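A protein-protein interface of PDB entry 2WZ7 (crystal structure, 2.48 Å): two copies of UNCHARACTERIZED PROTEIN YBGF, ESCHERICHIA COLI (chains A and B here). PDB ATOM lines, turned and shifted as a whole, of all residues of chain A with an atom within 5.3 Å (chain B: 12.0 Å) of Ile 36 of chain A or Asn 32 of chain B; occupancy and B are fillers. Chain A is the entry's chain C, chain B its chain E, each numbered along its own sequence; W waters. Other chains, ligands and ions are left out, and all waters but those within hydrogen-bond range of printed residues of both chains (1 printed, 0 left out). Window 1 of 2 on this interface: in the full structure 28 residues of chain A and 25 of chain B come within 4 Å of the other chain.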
ATOM      1  N   LEU A  29      -5.492 -32.491   7.122  1.00  0.00           N
ATOM      2  CA  LEU A  29      -5.364 -31.651   5.920  1.00  0.00           C
ATOM      3  C   LEU A  29      -4.769 -30.298   6.274  1.00  0.00           C
ATOM      4  O   LEU A  29      -3.855 -29.836   5.637  1.00  0.00           O
ATOM      5  CB  LEU A  29      -6.706 -31.519   5.170  1.00  0.00           C
ATOM      6  CG  LEU A  29      -7.077 -32.792   4.357  1.00  0.00           C
ATOM      7  CD1 LEU A  29      -8.497 -32.882   4.062  1.00  0.00           C
ATOM      8  CD2 LEU A  29      -6.310 -32.887   3.049  1.00  0.00           C
ATOM      9  N   ASP A  31      -3.002 -29.566   8.970  1.00  0.00           N
ATOM     10  CA  ASP A  31      -1.616 -29.806   9.370  1.00  0.00           C
ATOM     11  C   ASP A  31      -0.736 -29.906   8.127  1.00  0.00           C
ATOM     12  O   ASP A  31       0.364 -29.283   8.089  1.00  0.00           O
ATOM     13  CB  ASP A  31      -1.479 -31.074  10.218  1.00  0.00           C
ATOM     14  CG  ASP A  31      -1.739 -30.829  11.698  1.00  0.00           C
ATOM     15  OD1 ASP A  31      -2.002 -29.655  12.097  1.00  0.00           O
ATOM     16  OD2 ASP A  31      -1.692 -31.819  12.480  1.00  0.00           O
ATOM     17  N   ASN A  32      -1.198 -30.655   7.110  1.00  0.00           N
ATOM     18  CA  ASN A  32      -0.427 -30.830   5.844  1.00  0.00           C
ATOM     19  C   ASN A  32      -0.133 -29.575   5.048  1.00  0.00           C
ATOM     20  O   ASN A  32       0.949 -29.399   4.500  1.00  0.00           O
ATOM     21  CB  ASN A  32      -1.076 -31.905   4.960  1.00  0.00           C
ATOM     22  CG  ASN A  32      -0.892 -33.290   5.540  1.00  0.00           C
ATOM     23  OD1 ASN A  32       0.126 -33.583   6.198  1.00  0.00           O
ATOM     24  ND2 ASN A  32      -1.841 -34.126   5.334  1.00  0.00           N
ATOM     25  N   GLN A  33      -1.097 -28.686   5.026  1.00  0.00           N
ATOM     26  CA  GLN A  33      -0.949 -27.341   4.475  1.00  0.00           C
ATOM     27  C   GLN A  33       0.177 -26.591   5.131  1.00  0.00           C
ATOM     28  O   GLN A  33       0.996 -25.933   4.463  1.00  0.00           O
ATOM     29  CB  GLN A  33      -2.278 -26.608   4.693  1.00  0.00           C
ATOM     30  CG  GLN A  33      -2.307 -25.234   4.176  1.00  0.00           C
ATOM     31  CD  GLN A  33      -3.585 -24.530   4.516  1.00  0.00           C
ATOM     32  OE1 GLN A  33      -3.983 -24.500   5.668  1.00  0.00           O
ATOM     33  NE2 GLN A  33      -4.252 -23.982   3.515  1.00  0.00           N
ATOM     34  N   SER A  34       0.234 -26.684   6.458  1.00  0.00           N
ATOM     35  CA  SER A  34       1.301 -26.023   7.202  1.00  0.00           C
ATOM     36  C   SER A  34       2.634 -26.692   6.902  1.00  0.00           C
ATOM     37  O   SER A  34       3.646 -26.005   6.760  1.00  0.00           O
ATOM     38  CB  SER A  34       1.016 -26.047   8.715  1.00  0.00           C
ATOM     39  OG  SER A  34      -0.027 -25.135   9.045  1.00  0.00           O
ATOM     40  N   ASP A  35       2.643 -28.017   6.865  1.00  0.00           N
ATOM     41  CA  ASP A  35       3.862 -28.770   6.540  1.00  0.00           C
ATOM     42  C   ASP A  35       4.358 -28.286   5.191  1.00  0.00           C
ATOM     43  O   ASP A  35       5.551 -28.008   5.025  1.00  0.00           O
ATOM     44  CB  ASP A  35       3.607 -30.308   6.424  1.00  0.00           C
ATOM     45  CG  ASP A  35       3.072 -30.955   7.726  1.00  0.00           C
ATOM     46  OD1 ASP A  35       3.390 -30.499   8.841  1.00  0.00           O
ATOM     47  OD2 ASP A  35       2.340 -31.970   7.634  1.00  0.00           O
ATOM     48  N   ILE A  36       3.436 -28.198   4.224  1.00  0.00           N
ATOM     49  CA  ILE A  36       3.808 -27.736   2.908  1.00  0.00           C
ATOM     50  C   ILE A  36       4.366 -26.336   2.921  1.00  0.00           C
ATOM     51  O   ILE A  36       5.342 -26.079   2.240  1.00  0.00           O
ATOM     52  CB  ILE A  36       2.663 -27.852   1.904  1.00  0.00           C
ATOM     53  CG1 ILE A  36       2.422 -29.338   1.545  1.00  0.00           C
ATOM     54  CG2 ILE A  36       3.014 -27.052   0.640  1.00  0.00           C
ATOM     55  CD1 ILE A  36       0.924 -29.693   1.227  1.00  0.00           C
ATOM     56  N   ASP A  37       3.771 -25.443   3.715  1.00  0.00           N
ATOM     57  CA  ASP A  37       4.305 -24.082   3.874  1.00  0.00           C
ATOM     58  C   ASP A  37       5.774 -24.117   4.294  1.00  0.00           C
ATOM     59  O   ASP A  37       6.640 -23.451   3.684  1.00  0.00           O
ATOM     60  CB  ASP A  37       3.468 -23.256   4.888  1.00  0.00           C
ATOM     61  CG  ASP A  37       2.032 -23.029   4.417  1.00  0.00           C
ATOM     62  OD1 ASP A  37       1.728 -23.278   3.222  1.00  0.00           O
ATOM     63  OD2 ASP A  37       1.205 -22.627   5.257  1.00  0.00           O
ATOM     64  N   SER A  38       6.067 -24.918   5.328  1.00  0.00           N
ATOM     65  CA  SER A  38       7.458 -25.061   5.715  1.00  0.00           C
ATOM     66  C   SER A  38       8.354 -25.549   4.546  1.00  0.00           C
ATOM     67  O   SER A  38       9.459 -25.024   4.319  1.00  0.00           O
ATOM     68  CB  SER A  38       7.618 -25.974   6.946  1.00  0.00           C
ATOM     69  OG  SER A  38       9.015 -26.336   7.058  1.00  0.00           O
ATOM     70  N   LEU A  39       7.895 -26.557   3.807  1.00  0.00           N
ATOM     71  CA  LEU A  39       8.719 -27.123   2.754  1.00  0.00           C
ATOM     72  C   LEU A  39       8.993 -26.100   1.662  1.00  0.00           C
ATOM     73  O   LEU A  39      10.139 -25.990   1.207  1.00  0.00           O
ATOM     74  CB  LEU A  39       8.103 -28.406   2.197  1.00  0.00           C
ATOM     75  CG  LEU A  39       7.890 -29.551   3.201  1.00  0.00           C
ATOM     76  CD1 LEU A  39       7.271 -30.733   2.493  1.00  0.00           C
ATOM     77  CD2 LEU A  39       9.163 -29.952   3.892  1.00  0.00           C
ATOM     78  N   ARG A  40       7.958 -25.325   1.296  1.00  0.00           N
ATOM     79  CA  ARG A  40       8.085 -24.228   0.336  1.00  0.00           C
ATOM     80  C   ARG A  40       9.052 -23.175   0.821  1.00  0.00           C
ATOM     81  O   ARG A  40       9.854 -22.603   0.035  1.00  0.00           O
ATOM     82  CB  ARG A  40       6.741 -23.569   0.117  1.00  0.00           C
ATOM     83  CG  ARG A  40       6.773 -22.401  -0.936  1.00  0.00           C
ATOM     84  CD  ARG A  40       5.390 -21.739  -1.023  1.00  0.00           C
ATOM     85  NE  ARG A  40       4.293 -22.675  -1.281  1.00  0.00           N
ATOM     86  CZ  ARG A  40       3.399 -23.066  -0.380  1.00  0.00           C
ATOM     87  NH1 ARG A  40       3.391 -22.581   0.878  1.00  0.00           N
ATOM     88  NH2 ARG A  40       2.474 -23.935  -0.735  1.00  0.00           N
ATOM     89  N   GLY A  41       9.002 -22.925   2.124  1.00  0.00           N
ATOM     90  CA  GLY A  41       9.906 -21.968   2.750  1.00  0.00           C
ATOM     91  C   GLY A  41      11.330 -22.372   2.497  1.00  0.00           C
ATOM     92  O   GLY A  41      12.135 -21.579   2.089  1.00  0.00           O
ATOM     93  N   THR B  23     -16.958 -32.010   0.208  1.00  0.00           N
ATOM     94  CA  THR B  23     -16.541 -31.219  -0.950  1.00  0.00           C
ATOM     95  C   THR B  23     -15.380 -30.313  -0.573  1.00  0.00           C
ATOM     96  O   THR B  23     -14.406 -30.199  -1.299  1.00  0.00           O
ATOM     97  CB  THR B  23     -17.742 -30.432  -1.531  1.00  0.00           C
ATOM     98  OG1 THR B  23     -18.773 -31.365  -1.869  1.00  0.00           O
ATOM     99  CG2 THR B  23     -17.390 -29.649  -2.772  1.00  0.00           C
ATOM    100  N   GLN B  24     -15.458 -29.723   0.600  1.00  0.00           N
ATOM    101  CA  GLN B  24     -14.417 -28.828   1.088  1.00  0.00           C
ATOM    102  C   GLN B  24     -13.108 -29.554   1.360  1.00  0.00           C
ATOM    103  O   GLN B  24     -12.038 -29.026   1.026  1.00  0.00           O
ATOM    104  CB  GLN B  24     -14.892 -28.117   2.358  1.00  0.00           C
ATOM    105  CG  GLN B  24     -16.055 -27.147   2.159  1.00  0.00           C
ATOM    106  CD  GLN B  24     -16.585 -26.587   3.493  1.00  0.00           C
ATOM    107  OE1 GLN B  24     -15.879 -26.580   4.503  1.00  0.00           O
ATOM    108  NE2 GLN B  24     -17.835 -26.130   3.499  1.00  0.00           N
ATOM    109  N   LEU B  25     -13.157 -30.753   1.950  1.00  0.00           N
ATOM    110  CA  LEU B  25     -11.905 -31.509   2.167  1.00  0.00           C
ATOM    111  C   LEU B  25     -11.229 -32.033   0.911  1.00  0.00           C
ATOM    112  O   LEU B  25      -9.990 -32.085   0.851  1.00  0.00           O
ATOM    113  CB  LEU B  25     -12.066 -32.657   3.141  1.00  0.00           C
ATOM    114  CG  LEU B  25     -12.672 -32.342   4.489  1.00  0.00           C
ATOM    115  CD1 LEU B  25     -12.695 -33.644   5.239  1.00  0.00           C
ATOM    116  CD2 LEU B  25     -11.864 -31.280   5.216  1.00  0.00           C
ATOM    117  N   GLN B  26     -12.038 -32.391  -0.086  1.00  0.00           N
ATOM    118  CA  GLN B  26     -11.581 -32.764  -1.426  1.00  0.00           C
ATOM    119  C   GLN B  26     -10.769 -31.660  -1.987  1.00  0.00           C
ATOM    120  O   GLN B  26      -9.636 -31.868  -2.389  1.00  0.00           O
ATOM    121  CB  GLN B  26     -12.779 -33.033  -2.365  1.00  0.00           C
ATOM    122  CG  GLN B  26     -13.223 -34.494  -2.399  1.00  0.00           C
ATOM    123  CD  GLN B  26     -14.754 -34.737  -2.572  1.00  0.00           C
ATOM    124  OE1 GLN B  26     -15.300 -35.693  -1.994  1.00  0.00           O
ATOM    125  NE2 GLN B  26     -15.434 -33.901  -3.387  1.00  0.00           N
ATOM    126  N   GLN B  27     -11.343 -30.468  -1.963  1.00  0.00           N
ATOM    127  CA  GLN B  27     -10.680 -29.246  -2.398  1.00  0.00           C
ATOM    128  C   GLN B  27      -9.335 -29.059  -1.715  1.00  0.00           C
ATOM    129  O   GLN B  27      -8.312 -28.919  -2.385  1.00  0.00           O
ATOM    130  CB  GLN B  27     -11.589 -28.015  -2.175  1.00  0.00           C
ATOM    131  CG  GLN B  27     -11.074 -26.704  -2.834  1.00  0.00           C
ATOM    132  CD  GLN B  27     -10.698 -26.901  -4.298  1.00  0.00           C
ATOM    133  OE1 GLN B  27     -11.499 -27.408  -5.091  1.00  0.00           O
ATOM    134  NE2 GLN B  27      -9.462 -26.533  -4.661  1.00  0.00           N
ATOM    135  N   GLN B  28      -9.334 -29.093  -0.387  1.00  0.00           N
ATOM    136  CA  GLN B  28      -8.133 -28.874   0.410  1.00  0.00           C
ATOM    137  C   GLN B  28      -7.033 -29.898   0.108  1.00  0.00           C
ATOM    138  O   GLN B  28      -5.863 -29.542  -0.062  1.00  0.00           O
ATOM    139  CB  GLN B  28      -8.537 -28.861   1.891  1.00  0.00           C
ATOM    140  CG  GLN B  28      -9.418 -27.626   2.188  1.00  0.00           C
ATOM    141  CD  GLN B  28     -10.069 -27.621   3.556  1.00  0.00           C
ATOM    142  OE1 GLN B  28     -11.210 -27.186   3.683  1.00  0.00           O
ATOM    143  NE2 GLN B  28      -9.355 -28.085   4.580  1.00  0.00           N
ATOM    144  N   LEU B  29      -7.416 -31.168  -0.010  1.00  0.00           N
ATOM    145  CA  LEU B  29      -6.515 -32.189  -0.518  1.00  0.00           C
ATOM    146  C   LEU B  29      -5.954 -31.889  -1.959  1.00  0.00           C
ATOM    147  O   LEU B  29      -4.721 -31.949  -2.170  1.00  0.00           O
ATOM    148  CB  LEU B  29      -7.239 -33.519  -0.469  1.00  0.00           C
ATOM    149  CG  LEU B  29      -6.453 -34.698  -0.962  1.00  0.00           C
ATOM    150  CD1 LEU B  29      -5.051 -34.770  -0.232  1.00  0.00           C
ATOM    151  CD2 LEU B  29      -7.343 -35.892  -0.731  1.00  0.00           C
ATOM    152  N   SER B  30      -6.809 -31.526  -2.926  1.00  0.00           N
ATOM    153  CA  SER B  30      -6.271 -31.140  -4.245  1.00  0.00           C
ATOM    154  C   SER B  30      -5.276 -30.010  -4.182  1.00  0.00           C
ATOM    155  O   SER B  30      -4.246 -30.055  -4.884  1.00  0.00           O
ATOM    156  CB  SER B  30      -7.358 -30.709  -5.218  1.00  0.00           C
ATOM    157  OG  SER B  30      -8.479 -31.535  -5.085  1.00  0.00           O
ATOM    158  N   ASP B  31      -5.592 -28.974  -3.391  1.00  0.00           N
ATOM    159  CA  ASP B  31      -4.645 -27.885  -3.168  1.00  0.00           C
ATOM    160  C   ASP B  31      -3.294 -28.448  -2.615  1.00  0.00           C
ATOM    161  O   ASP B  31      -2.230 -28.100  -3.106  1.00  0.00           O
ATOM    162  CB  ASP B  31      -5.224 -26.813  -2.247  1.00  0.00           C
ATOM    163  CG  ASP B  31      -6.474 -26.114  -2.825  1.00  0.00           C
ATOM    164  OD1 ASP B  31      -6.720 -26.153  -4.049  1.00  0.00           O
ATOM    165  OD2 ASP B  31      -7.225 -25.497  -2.045  1.00  0.00           O
ATOM    166  N   ASN B  32      -3.345 -29.357  -1.627  1.00  0.00           N
ATOM    167  CA  ASN B  32      -2.116 -29.990  -1.132  1.00  0.00           C
ATOM    168  C   ASN B  32      -1.408 -30.797  -2.207  1.00  0.00           C
ATOM    169  O   ASN B  32      -0.206 -30.708  -2.307  1.00  0.00           O
ATOM    170  CB  ASN B  32      -2.372 -30.808   0.149  1.00  0.00           C
ATOM    171  CG  ASN B  32      -2.795 -29.925   1.337  1.00  0.00           C
ATOM    172  OD1 ASN B  32      -2.566 -28.706   1.347  1.00  0.00           O
ATOM    173  ND2 ASN B  32      -3.370 -30.542   2.348  1.00  0.00           N
ATOM    174  N   GLN B  33      -2.125 -31.516  -3.054  1.00  0.00           N
ATOM    175  CA  GLN B  33      -1.448 -32.231  -4.170  1.00  0.00           C
ATOM    176  C   GLN B  33      -0.816 -31.267  -5.136  1.00  0.00           C
ATOM    177  O   GLN B  33       0.378 -31.319  -5.364  1.00  0.00           O
ATOM    178  CB  GLN B  33      -2.363 -33.249  -4.898  1.00  0.00           C
ATOM    179  CG  GLN B  33      -3.032 -34.220  -3.910  1.00  0.00           C
ATOM    180  CD  GLN B  33      -4.146 -35.153  -4.482  1.00  0.00           C
ATOM    181  OE1 GLN B  33      -5.249 -34.706  -4.911  1.00  0.00           O
ATOM    182  NE2 GLN B  33      -3.879 -36.473  -4.406  1.00  0.00           N
ATOM    183  N   SER B  34      -1.592 -30.330  -5.657  1.00  0.00           N
ATOM    184  CA  SER B  34      -0.996 -29.275  -6.512  1.00  0.00           C
ATOM    185  C   SER B  34       0.207 -28.582  -5.949  1.00  0.00           C
ATOM    186  O   SER B  34       1.190 -28.416  -6.642  1.00  0.00           O
ATOM    187  CB  SER B  34      -2.032 -28.242  -6.955  1.00  0.00           C
ATOM    188  OG  SER B  34      -2.986 -28.926  -7.722  1.00  0.00           O
ATOM    189  N   ASP B  35       0.169 -28.194  -4.683  1.00  0.00           N
ATOM    190  CA  ASP B  35       1.337 -27.561  -4.120  1.00  0.00           C
ATOM    191  C   ASP B  35       2.557 -28.481  -4.057  1.00  0.00           C
ATOM    192  O   ASP B  35       3.639 -28.016  -4.309  1.00  0.00           O
ATOM    193  CB  ASP B  35       1.032 -26.940  -2.769  1.00  0.00           C
ATOM    194  CG  ASP B  35       0.090 -25.759  -2.874  1.00  0.00           C
ATOM    195  OD1 ASP B  35      -0.024 -25.194  -3.970  1.00  0.00           O
ATOM    196  OD2 ASP B  35      -0.535 -25.386  -1.872  1.00  0.00           O
ATOM    197  N   ILE B  36       2.377 -29.774  -3.753  1.00  0.00           N
ATOM    198  CA  ILE B  36       3.462 -30.769  -3.772  1.00  0.00           C
ATOM    199  C   ILE B  36       4.058 -30.937  -5.143  1.00  0.00           C
ATOM    200  O   ILE B  36       5.296 -30.916  -5.281  1.00  0.00           O
ATOM    201  CB  ILE B  36       3.004 -32.206  -3.291  1.00  0.00           C
ATOM    202  CG1 ILE B  36       2.597 -32.191  -1.816  1.00  0.00           C
ATOM    203  CG2 ILE B  36       4.133 -33.261  -3.495  1.00  0.00           C
ATOM    204  CD1 ILE B  36       3.764 -32.040  -0.888  1.00  0.00           C
ATOM    205  N   ASP B  37       3.219 -31.114  -6.166  1.00  0.00           N
ATOM    206  CA  ASP B  37       3.754 -31.347  -7.528  1.00  0.00           C
ATOM    207  C   ASP B  37       4.592 -30.147  -7.985  1.00  0.00           C
ATOM    208  O   ASP B  37       5.743 -30.284  -8.419  1.00  0.00           O
ATOM    209  CB  ASP B  37       2.617 -31.684  -8.514  1.00  0.00           C
ATOM    210  CG  ASP B  37       1.799 -32.941  -8.075  1.00  0.00           C
ATOM    211  OD1 ASP B  37       2.340 -33.795  -7.297  1.00  0.00           O
ATOM    212  OD2 ASP B  37       0.613 -33.086  -8.513  1.00  0.00           O
ATOM    213  N   SER B  38       4.020 -28.955  -7.833  1.00  0.00           N
ATOM    214  CA  SER B  38       4.756 -27.706  -8.058  1.00  0.00           C
ATOM    215  C   SER B  38       6.124 -27.690  -7.339  1.00  0.00           C
ATOM    216  O   SER B  38       7.185 -27.444  -7.954  1.00  0.00           O
ATOM    217  CB  SER B  38       3.894 -26.519  -7.597  1.00  0.00           C
ATOM    218  OG  SER B  38       4.601 -25.337  -7.824  1.00  0.00           O
ATOM    219  N   LEU B  39       6.099 -27.952  -6.033  1.00  0.00           N
ATOM    220  CA  LEU B  39       7.317 -27.932  -5.253  1.00  0.00           C
ATOM    221  C   LEU B  39       8.331 -29.041  -5.728  1.00  0.00           C
ATOM    222  O   LEU B  39       9.522 -28.778  -5.836  1.00  0.00           O
ATOM    223  CB  LEU B  39       6.978 -28.010  -3.757  1.00  0.00           C
ATOM    224  CG  LEU B  39       6.360 -26.861  -2.956  1.00  0.00           C
ATOM    225  CD1 LEU B  39       6.424 -27.218  -1.454  1.00  0.00           C
ATOM    226  CD2 LEU B  39       7.029 -25.467  -3.173  1.00  0.00           C
ATOM    227  N   ARG B  40       7.866 -30.251  -6.029  1.00  0.00           N
ATOM    228  CA  ARG B  40       8.745 -31.219  -6.726  1.00  0.00           C
ATOM    229  C   ARG B  40       9.452 -30.637  -7.961  1.00  0.00           C
ATOM    230  O   ARG B  40      10.706 -30.728  -8.051  1.00  0.00           O
ATOM    231  CB  ARG B  40       8.001 -32.495  -7.118  1.00  0.00           C
ATOM    232  CG  ARG B  40       7.580 -33.341  -5.920  1.00  0.00           C
ATOM    233  CD  ARG B  40       6.926 -34.664  -6.342  1.00  0.00           C
ATOM    234  NE  ARG B  40       7.825 -35.531  -7.118  1.00  0.00           N
ATOM    235  CZ  ARG B  40       7.480 -36.743  -7.552  1.00  0.00           C
ATOM    236  NH1 ARG B  40       8.352 -37.459  -8.265  1.00  0.00           N
ATOM    237  NH2 ARG B  40       6.271 -37.235  -7.271  1.00  0.00           N
ATOM    238  N   GLY B  41       8.696 -30.011  -8.882  1.00  0.00           N
ATOM    239  CA  GLY B  41       9.303 -29.343 -10.049  1.00  0.00           C
ATOM    240  C   GLY B  41      10.457 -28.413  -9.685  1.00  0.00           C
ATOM    241  O   GLY B  41      11.560 -28.499 -10.263  1.00  0.00           O
ATOM    242  N   GLN B  42      10.233 -27.546  -8.705  1.00  0.00           N
ATOM    243  CA  GLN B  42      11.232 -26.550  -8.322  1.00  0.00           C
ATOM    244  C   GLN B  42      12.491 -27.158  -7.694  1.00  0.00           C
ATOM    245  O   GLN B  42      13.618 -26.722  -7.997  1.00  0.00           O
ATOM    246  CB  GLN B  42      10.609 -25.499  -7.383  1.00  0.00           C
ATOM    247  CG  GLN B  42       9.314 -24.907  -7.909  1.00  0.00           C
ATOM    248  CD  GLN B  42       8.573 -24.127  -6.848  1.00  0.00           C
ATOM    249  OE1 GLN B  42       9.106 -23.891  -5.759  1.00  0.00           O
ATOM    250  NE2 GLN B  42       7.330 -23.725  -7.152  1.00  0.00           N
ATOM    251  N   ILE B  43      12.307 -28.147  -6.820  1.00  0.00           N
ATOM    252  CA  ILE B  43      13.461 -28.854  -6.207  1.00  0.00           C
ATOM    253  C   ILE B  43      14.298 -29.603  -7.275  1.00  0.00           C
ATOM    254  O   ILE B  43      15.520 -29.524  -7.247  1.00  0.00           O
ATOM    255  CB  ILE B  43      13.097 -29.695  -4.915  1.00  0.00           C
ATOM    256  CG1 ILE B  43      14.368 -30.187  -4.168  1.00  0.00           C
ATOM    257  CG2 ILE B  43      12.264 -30.869  -5.262  1.00  0.00           C
ATOM    258  CD1 ILE B  43      15.151 -29.093  -3.472  1.00  0.00           C
HETATM  259  O   HOH W   1      -2.737 -33.446   2.849  1.00  0.00           O
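Among the printed residues, pairs that only touch across the chains: Ile 36 of chain A with Asn 32 of chain B (3.6 Å), Leu 29 of chain A with Leu 25 of chain B (3.6 Å), Leu 29 of chain A with Leu 29 of chain B (3.6 Å), Arg 40 of chain A with Leu 39 of chain B (3.7 Å), Asn 32 of chain A with Asn 32 of chain B (3.7 Å), Gln 33 of chain A with Asn 32 of chain B (3.8 Å), Ile 36 of chain A with Ile 36 of chain B (3.9 Å) and Ile 36 of chain A with Asp 35 of chain B (3.9 Å).
The backbone carbonyl oxygen (O) of Leu 29 of chain A sits at hydrogen-bond distance from the side-chain amide nitrogen (ND2) of Asn 32 of chain B (3.4 Å).
NH2 of Arg 40 of chain A is in salt-bridge range of OD2 of Asp 35 of chain B (3.5 Å).
Leu 29 of chain B touches its own counterpart, Leu 29 of chain A.
Gln 33 of chain A touches Asn 32 of chain B, but with the chains exchanged Asn 32 of chain A does not touch Gln 33 of chain B (8.1 Å).
Arg 40 of chain A touches Asp 35 of chain B, but with the chains exchanged Asp 35 of chain A does not touch Arg 40 of chain B (11.5 Å).
Arg 40 of chain A touches Leu 39 of chain B, but with the chains exchanged Leu 39 of chain A does not touch Arg 40 of chain B (8.4 Å).
12 positions are printed for both chains.
Of the 21 printed residues of chain B, 6 touch a printed residue of chain A.
Printed residues of chain B that touch a printed residue of chain A: Leu 25, Leu 29, Asn 32, Asp 35, Ile 36 and Leu 39.
Hydrophobic or aromatic side chains of chain B that line the printed part of chain A: Leu 25, Leu 29, Ile 36 and Leu 39.
Hydrophobic or aromatic side chains of chain A within 4 Å of the printed part of chain B: Leu 29 and Ile 36.
OD2 of Asp 35 of chain A sits close to OD1 of Asn 32 of chain A.
The side-chain carboxylate (OD1) of Asp 37 of chain A lies within salt-bridge range of the guanidinium group (NH1) of Arg 40 of chain A (3.0 Å).
Water W1 bridges ND2 of Asn 32 of chain A and ND2 of Asn 32 of chain B.
Of chain B, only Asn 32 comes within 4 Å of Asn 32 of chain A.
No residue of chain B comes within 4 Å of Asp 35 of chain A.
Of the printed residues of chain B, Ile 36 of chain A touches Asn 32, Asp 35 and Ile 36.
No residue of chain B comes within 4 Å of Ser 38 of chain A.
No residue of chain B comes within 4 Å of Leu 39 of chain A.
Of the printed residues of chain A, Leu 29 of chain B touches Leu 29 (3.6 Å).
Of chain A, only Leu 29, Asn 32, Gln 33 and Ile 36 come within 4 Å of Asn 32 of chain B.
Of the printed residues of chain A, Asp 35 of chain B touches Ile 36 (3.9 Å) and Arg 40 (3.5 Å).
Of the printed residues of chain A, Ile 36 of chain B touches Ile 36.
The nearest printed residue of chain B that does not touch Ile 36 of chain A is Leu 39 of chain B (4.01 Å).
The nearest printed residue of chain A that does not touch Asn 32 of chain B is Ser 34 of chain A (6.2 Å).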
